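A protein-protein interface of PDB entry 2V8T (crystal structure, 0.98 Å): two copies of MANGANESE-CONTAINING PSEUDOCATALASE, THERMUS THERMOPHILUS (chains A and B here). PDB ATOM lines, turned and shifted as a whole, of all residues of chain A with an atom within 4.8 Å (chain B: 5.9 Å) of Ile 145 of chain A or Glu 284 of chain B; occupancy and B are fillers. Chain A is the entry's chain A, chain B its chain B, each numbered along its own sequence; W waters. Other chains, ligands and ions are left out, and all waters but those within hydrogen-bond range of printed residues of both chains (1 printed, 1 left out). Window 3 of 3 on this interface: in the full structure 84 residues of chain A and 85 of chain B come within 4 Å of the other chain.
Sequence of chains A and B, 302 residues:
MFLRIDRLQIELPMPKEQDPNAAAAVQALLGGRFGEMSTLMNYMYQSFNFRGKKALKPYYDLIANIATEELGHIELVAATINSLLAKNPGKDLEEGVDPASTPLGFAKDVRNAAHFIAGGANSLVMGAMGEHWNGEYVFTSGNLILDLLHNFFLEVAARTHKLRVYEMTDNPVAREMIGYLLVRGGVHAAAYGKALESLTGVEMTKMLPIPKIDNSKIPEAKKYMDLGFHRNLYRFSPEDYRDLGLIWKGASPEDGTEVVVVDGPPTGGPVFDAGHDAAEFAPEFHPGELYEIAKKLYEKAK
O of Pro 283 of chain B touches CA of Asn 143 of chain A, 3.5 Å away. CD1 of Ile 145 of chain A touches OE2 of Glu 284 of chain B, 3.9 Å away. Leu 290 of chain B touches Leu 199 of chain A (CD2 to CD2, 3.9 Å).
Printed residues of chain B within 4 Å of Asn 143 of chain A: Phe 281 (2.8 Å), Pro 283 (3.5 Å) and Glu 284 (3.3 Å). Of the printed residues of chain B, Leu 144 of chain A touches Pro 283 (3.0 Å). Ile 145 of chain A touches one residue of chain B. Of the printed residues of chain B, Leu 199 of chain A touches Leu 290 (3.9 Å). Of the printed residues of chain A, Phe 281 of chain B touches Asn 143 (2.8 Å). Glu 284 of chain B touches two residues of chain A. Printed residues of chain A within 4 Å of Leu 290 of chain B: Leu 199. The nearest printed residue of chain A that does not touch Pro 283 of chain B is Ile 145 of chain A (4.8 Å).
Water W1 bridges the side-chain carboxylate of Glu 284 of chain B (2.7 Å) and the side-chain amide oxygen of Asn 143 of chain A (2.9 Å).
No position is printed for both chains.
O of Pro 283 of chain B sits at hydrogen-bond distance from N of Leu 144 of chain A, at 3.0 Å. ND2 of Asn 143 of chain A is in hydrogen-bond range of O of Phe 281 of chain B, 2.8 Å away. The side-chain carboxylate (OE1) of Glu 284 of chain B sits at hydrogen-bond distance from the side-chain amide nitrogen (ND2) of Asn 143 of chain A (3.3 Å).
Hydrophobic or aromatic side chains of chain B within 4 Å of the printed part of chain A: Phe 281 and Leu 290. Hydrophobic or aromatic side chains of chain A within 4 Å of the printed part of chain B: Leu 144, Ile 145 and Leu 199. Among the printed residues, no Asp or Glu carboxylate lies within 4 Å of a Lys or Arg side-chain nitrogen of the other chain.
A ring nitrogen (NE2) of His 276 of chain B lies within hydrogen-bond range of the backbone carbonyl oxygen (O) of Glu 284 of chain B. The backbone NH (N) of Leu 146 of chain A is in hydrogen-bond range of the side-chain amide oxygen (OD1) of Asn 143 of chain A, at 3.0 Å. The side-chain amide oxygen (OD1) of Asn 143 of chain A lies close to the backbone NH (N) of Ile 145 of chain A, at 3.5 Å.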
ATOM      1  N   ASN A 143      -8.035  -2.550  -8.566  1.00  0.00           N
ATOM      2  CA  ASN A 143      -8.581  -1.886  -7.387  1.00  0.00           C
ATOM      3  C   ASN A 143     -10.054  -1.600  -7.651  1.00  0.00           C
ATOM      4  O   ASN A 143     -10.401  -0.902  -8.615  1.00  0.00           O
ATOM      5  CB  ASN A 143      -7.828  -0.586  -7.099  1.00  0.00           C
ATOM      6  CG  ASN A 143      -8.327   0.154  -5.878  1.00  0.00           C
ATOM      7  OD1 ASN A 143      -9.286   0.934  -5.941  1.00  0.00           O
ATOM      8  ND2 ASN A 143      -7.708  -0.122  -4.733  1.00  0.00           N
ATOM      9  N   LEU A 144     -10.937  -2.194  -6.841  1.00  0.00           N
ATOM     10  CA  LEU A 144     -12.366  -2.142  -7.144  1.00  0.00           C
ATOM     11  C   LEU A 144     -12.913  -0.729  -7.233  1.00  0.00           C
ATOM     12  O   LEU A 144     -13.636  -0.403  -8.178  1.00  0.00           O
ATOM     13  CB  LEU A 144     -13.137  -2.994  -6.097  1.00  0.00           C
ATOM     14  CG  LEU A 144     -14.639  -2.995  -6.301  1.00  0.00           C
ATOM     15  CD1 LEU A 144     -15.038  -3.505  -7.669  1.00  0.00           C
ATOM     16  CD2 LEU A 144     -15.285  -3.835  -5.193  1.00  0.00           C
ATOM     17  N   ILE A 145     -12.631   0.099  -6.217  1.00  0.00           N
ATOM     18  CA  ILE A 145     -13.217   1.433  -6.219  1.00  0.00           C
ATOM     19  C   ILE A 145     -12.683   2.272  -7.405  1.00  0.00           C
ATOM     20  O   ILE A 145     -13.443   2.986  -8.049  1.00  0.00           O
ATOM     21  CB  ILE A 145     -13.019   2.121  -4.865  1.00  0.00           C
ATOM     22  CG1 ILE A 145     -13.924   1.421  -3.822  1.00  0.00           C
ATOM     23  CG2 ILE A 145     -13.326   3.614  -4.958  1.00  0.00           C
ATOM     24  CD1 ILE A 145     -13.572   1.776  -2.394  1.00  0.00           C
ATOM     25  N   LEU A 146     -11.381   2.187  -7.656  1.00  0.00           N
ATOM     26  CA  LEU A 146     -10.781   2.933  -8.789  1.00  0.00           C
ATOM     27  C   LEU A 146     -11.429   2.496 -10.113  1.00  0.00           C
ATOM     28  O   LEU A 146     -11.763   3.336 -10.952  1.00  0.00           O
ATOM     29  CB  LEU A 146      -9.291   2.722  -8.761  1.00  0.00           C
ATOM     30  CG  LEU A 146      -8.482   3.520  -9.821  1.00  0.00           C
ATOM     31  CD1 LEU A 146      -8.621   5.005  -9.670  1.00  0.00           C
ATOM     32  CD2 LEU A 146      -7.026   3.085  -9.723  1.00  0.00           C
ATOM     33  N   ASP A 147     -11.591   1.192 -10.295  1.00  0.00           N
ATOM     34  CA  ASP A 147     -12.225   0.678 -11.502  1.00  0.00           C
ATOM     35  C   ASP A 147     -13.683   1.162 -11.621  1.00  0.00           C
ATOM     36  O   ASP A 147     -14.127   1.538 -12.700  1.00  0.00           O
ATOM     37  CB  ASP A 147     -12.209  -0.842 -11.541  1.00  0.00           C
ATOM     38  CG  ASP A 147     -10.823  -1.466 -11.918  1.00  0.00           C
ATOM     39  OD1 ASP A 147      -9.888  -0.759 -12.283  1.00  0.00           O
ATOM     40  OD2 ASP A 147     -10.831  -2.717 -11.843  1.00  0.00           O
ATOM     41  N   LEU A 148     -14.433   1.126 -10.505  1.00  0.00           N
ATOM     42  CA  LEU A 148     -15.814   1.560 -10.574  1.00  0.00           C
ATOM     43  C   LEU A 148     -15.956   3.041 -10.854  1.00  0.00           C
ATOM     44  O   LEU A 148     -16.858   3.472 -11.560  1.00  0.00           O
ATOM     45  CB  LEU A 148     -16.564   1.211  -9.261  1.00  0.00           C
ATOM     46  CG  LEU A 148     -16.864  -0.276  -9.076  1.00  0.00           C
ATOM     47  CD1 LEU A 148     -17.323  -0.512  -7.637  1.00  0.00           C
ATOM     48  CD2 LEU A 148     -17.969  -0.722 -10.059  1.00  0.00           C
ATOM     49  N   LEU A 149     -15.053   3.865 -10.274  1.00  0.00           N
ATOM     50  CA  LEU A 149     -15.024   5.288 -10.569  1.00  0.00           C
ATOM     51  C   LEU A 149     -14.774   5.503 -12.072  1.00  0.00           C
ATOM     52  O   LEU A 149     -15.457   6.278 -12.735  1.00  0.00           O
ATOM     53  CB  LEU A 149     -13.951   5.961  -9.697  1.00  0.00           C
ATOM     54  CG  LEU A 149     -13.744   7.432  -9.977  1.00  0.00           C
ATOM     55  CD1 LEU A 149     -14.983   8.285  -9.713  1.00  0.00           C
ATOM     56  CD2 LEU A 149     -12.536   7.945  -9.140  1.00  0.00           C
ATOM     57  N   LEU A 196     -20.737   2.480  -6.180  1.00  0.00           N
ATOM     58  CA  LEU A 196     -19.838   3.416  -5.480  1.00  0.00           C
ATOM     59  C   LEU A 196     -20.487   3.945  -4.215  1.00  0.00           C
ATOM     60  O   LEU A 196     -19.783   4.096  -3.190  1.00  0.00           O
ATOM     61  CB  LEU A 196     -19.458   4.567  -6.410  1.00  0.00           C
ATOM     62  CG  LEU A 196     -18.434   4.203  -7.477  1.00  0.00           C
ATOM     63  CD1 LEU A 196     -18.434   5.216  -8.610  1.00  0.00           C
ATOM     64  CD2 LEU A 196     -17.060   4.021  -6.861  1.00  0.00           C
ATOM     65  N   LEU A 199     -19.977   1.369  -1.477  1.00  0.00           N
ATOM     66  CA  LEU A 199     -18.603   1.166  -1.050  1.00  0.00           C
ATOM     67  C   LEU A 199     -17.979   2.384  -0.376  1.00  0.00           C
ATOM     68  O   LEU A 199     -16.999   2.215   0.370  1.00  0.00           O
ATOM     69  CB  LEU A 199     -17.757   0.750  -2.244  1.00  0.00           C
ATOM     70  CG  LEU A 199     -18.039  -0.625  -2.781  1.00  0.00           C
ATOM     71  CD1 LEU A 199     -17.446  -0.698  -4.252  1.00  0.00           C
ATOM     72  CD2 LEU A 199     -17.530  -1.735  -1.863  1.00  0.00           C
ATOM     73  N   THR A 200     -18.465   3.570  -0.693  1.00  0.00           N
ATOM     74  CA  THR A 200     -17.806   4.805  -0.320  1.00  0.00           C
ATOM     75  C   THR A 200     -18.692   5.802   0.451  1.00  0.00           C
ATOM     76  O   THR A 200     -18.164   6.752   1.047  1.00  0.00           O
ATOM     77  CB  THR A 200     -17.256   5.586  -1.551  1.00  0.00           C
ATOM     78  OG1 THR A 200     -18.308   6.221  -2.257  1.00  0.00           O
ATOM     79  CG2 THR A 200     -16.406   4.725  -2.486  1.00  0.00           C
ATOM     80  N   HIS B 276      -5.970 -11.617  -2.750  1.00  0.00           N
ATOM     81  CA  HIS B 276      -5.511 -10.303  -2.360  1.00  0.00           C
ATOM     82  C   HIS B 276      -4.042 -10.126  -2.682  1.00  0.00           C
ATOM     83  O   HIS B 276      -3.223 -11.020  -2.375  1.00  0.00           O
ATOM     84  CB  HIS B 276      -5.746 -10.157  -0.856  1.00  0.00           C
ATOM     85  CG  HIS B 276      -5.373  -8.827  -0.286  1.00  0.00           C
ATOM     86  ND1 HIS B 276      -4.981  -8.724   1.029  1.00  0.00           N
ATOM     87  CD2 HIS B 276      -5.379  -7.568  -0.820  1.00  0.00           C
ATOM     88  CE1 HIS B 276      -4.738  -7.451   1.246  1.00  0.00           C
ATOM     89  NE2 HIS B 276      -4.970  -6.719   0.156  1.00  0.00           N
ATOM     90  N   ASP B 277      -3.678  -8.988  -3.257  1.00  0.00           N
ATOM     91  CA  ASP B 277      -2.287  -8.568  -3.445  1.00  0.00           C
ATOM     92  C   ASP B 277      -2.217  -7.135  -2.905  1.00  0.00           C
ATOM     93  O   ASP B 277      -2.590  -6.167  -3.599  1.00  0.00           O
ATOM     94  CB  ASP B 277      -1.840  -8.691  -4.898  1.00  0.00           C
ATOM     95  CG  ASP B 277      -0.396  -8.386  -5.139  1.00  0.00           C
ATOM     96  OD1 ASP B 277       0.191  -7.590  -4.352  1.00  0.00           O
ATOM     97  OD2 ASP B 277       0.147  -8.885  -6.165  1.00  0.00           O
ATOM     98  N   ALA B 278      -1.828  -7.002  -1.630  1.00  0.00           N
ATOM     99  CA  ALA B 278      -1.873  -5.704  -0.980  1.00  0.00           C
ATOM    100  C   ALA B 278      -0.962  -4.695  -1.653  1.00  0.00           C
ATOM    101  O   ALA B 278      -1.325  -3.499  -1.749  1.00  0.00           O
ATOM    102  CB  ALA B 278      -1.466  -5.841   0.496  1.00  0.00           C
ATOM    103  N   PHE B 281      -2.712  -3.084  -4.222  1.00  0.00           N
ATOM    104  CA  PHE B 281      -3.945  -2.440  -3.782  1.00  0.00           C
ATOM    105  C   PHE B 281      -5.150  -3.143  -4.414  1.00  0.00           C
ATOM    106  O   PHE B 281      -6.159  -2.487  -4.743  1.00  0.00           O
ATOM    107  CB  PHE B 281      -3.955  -0.945  -4.037  1.00  0.00           C
ATOM    108  CG  PHE B 281      -2.619  -0.303  -3.719  1.00  0.00           C
ATOM    109  CD1 PHE B 281      -2.119  -0.290  -2.437  1.00  0.00           C
ATOM    110  CD2 PHE B 281      -1.814   0.221  -4.724  1.00  0.00           C
ATOM    111  CE1 PHE B 281      -0.854   0.233  -2.142  1.00  0.00           C
ATOM    112  CE2 PHE B 281      -0.559   0.718  -4.451  1.00  0.00           C
ATOM    113  CZ  PHE B 281      -0.062   0.707  -3.152  1.00  0.00           C
ATOM    114  N   ALA B 282      -5.089  -4.466  -4.527  1.00  0.00           N
ATOM    115  CA  ALA B 282      -6.041  -5.211  -5.357  1.00  0.00           C
ATOM    116  C   ALA B 282      -6.580  -6.382  -4.542  1.00  0.00           C
ATOM    117  O   ALA B 282      -5.824  -7.258  -4.128  1.00  0.00           O
ATOM    118  CB  ALA B 282      -5.322  -5.693  -6.632  1.00  0.00           C
ATOM    119  N   PRO B 283      -7.890  -6.407  -4.243  1.00  0.00           N
ATOM    120  CA  PRO B 283      -8.933  -5.465  -4.689  1.00  0.00           C
ATOM    121  C   PRO B 283      -8.959  -4.147  -3.907  1.00  0.00           C
ATOM    122  O   PRO B 283      -9.648  -3.218  -4.333  1.00  0.00           O
ATOM    123  CB  PRO B 283     -10.225  -6.278  -4.470  1.00  0.00           C
ATOM    124  CG  PRO B 283      -9.905  -7.133  -3.260  1.00  0.00           C
ATOM    125  CD  PRO B 283      -8.459  -7.509  -3.420  1.00  0.00           C
ATOM    126  N   GLU B 284      -8.231  -4.104  -2.800  1.00  0.00           N
ATOM    127  CA  GLU B 284      -8.015  -2.898  -2.008  1.00  0.00           C
ATOM    128  C   GLU B 284      -6.720  -3.142  -1.225  1.00  0.00           C
ATOM    129  O   GLU B 284      -6.288  -4.287  -1.094  1.00  0.00           O
ATOM    130  CB  GLU B 284      -9.223  -2.648  -1.063  1.00  0.00           C
ATOM    131  CG  GLU B 284      -9.193  -1.329  -0.286  1.00  0.00           C
ATOM    132  CD  GLU B 284      -8.960  -0.142  -1.185  1.00  0.00           C
ATOM    133  OE1 GLU B 284      -7.788   0.179  -1.497  1.00  0.00           O
ATOM    134  OE2 GLU B 284     -10.027   0.454  -1.620  1.00  0.00           O
ATOM    135  N   PHE B 285      -6.116  -2.061  -0.699  1.00  0.00           N
ATOM    136  CA  PHE B 285      -4.918  -2.239   0.121  1.00  0.00           C
ATOM    137  C   PHE B 285      -5.193  -3.212   1.290  1.00  0.00           C
ATOM    138  O   PHE B 285      -4.510  -4.219   1.461  1.00  0.00           O
ATOM    139  CB  PHE B 285      -4.450  -0.885   0.624  1.00  0.00           C
ATOM    140  CG  PHE B 285      -3.192  -0.947   1.466  1.00  0.00           C
ATOM    141  CD1 PHE B 285      -2.079  -1.648   1.073  1.00  0.00           C
ATOM    142  CD2 PHE B 285      -3.140  -0.300   2.672  1.00  0.00           C
ATOM    143  CE1 PHE B 285      -0.921  -1.695   1.858  1.00  0.00           C
ATOM    144  CE2 PHE B 285      -2.012  -0.351   3.449  1.00  0.00           C
ATOM    145  CZ  PHE B 285      -0.892  -1.053   3.057  1.00  0.00           C
ATOM    146  N   HIS B 286      -6.223  -2.886   2.096  1.00  0.00           N
ATOM    147  CA  HIS B 286      -6.702  -3.706   3.237  1.00  0.00           C
ATOM    148  C   HIS B 286      -8.192  -3.924   2.979  1.00  0.00           C
ATOM    149  O   HIS B 286      -8.993  -3.060   3.316  1.00  0.00           O
ATOM    150  CB  HIS B 286      -6.477  -2.944   4.563  1.00  0.00           C
ATOM    151  CG  HIS B 286      -5.041  -2.793   4.929  1.00  0.00           C
ATOM    152  ND1 HIS B 286      -4.604  -1.862   5.848  1.00  0.00           N
ATOM    153  CD2 HIS B 286      -3.939  -3.475   4.545  1.00  0.00           C
ATOM    154  CE1 HIS B 286      -3.302  -2.013   6.042  1.00  0.00           C
ATOM    155  NE2 HIS B 286      -2.862  -2.981   5.259  1.00  0.00           N
ATOM    156  N   PRO B 287      -8.610  -5.063   2.372  1.00  0.00           N
ATOM    157  CA  PRO B 287      -9.995  -5.187   1.874  1.00  0.00           C
ATOM    158  C   PRO B 287     -11.013  -5.600   2.916  1.00  0.00           C
ATOM    159  O   PRO B 287     -12.169  -5.787   2.566  1.00  0.00           O
ATOM    160  CB  PRO B 287      -9.869  -6.267   0.785  1.00  0.00           C
ATOM    161  CG  PRO B 287      -8.691  -7.139   1.306  1.00  0.00           C
ATOM    162  CD  PRO B 287      -7.721  -6.152   1.912  1.00  0.00           C
ATOM    163  N   LEU B 290     -14.273  -3.595   2.971  1.00  0.00           N
ATOM    164  CA  LEU B 290     -15.129  -3.834   1.810  1.00  0.00           C
ATOM    165  C   LEU B 290     -15.798  -5.203   1.887  1.00  0.00           C
ATOM    166  O   LEU B 290     -16.957  -5.332   1.520  1.00  0.00           O
ATOM    167  CB  LEU B 290     -14.368  -3.678   0.492  1.00  0.00           C
ATOM    168  CG  LEU B 290     -13.696  -2.330   0.268  1.00  0.00           C
ATOM    169  CD1 LEU B 290     -13.204  -2.233  -1.175  1.00  0.00           C
ATOM    170  CD2 LEU B 290     -14.579  -1.138   0.622  1.00  0.00           C
HETATM  171  O   HOH W   1      -9.543   2.392  -3.488  1.00  0.00           O
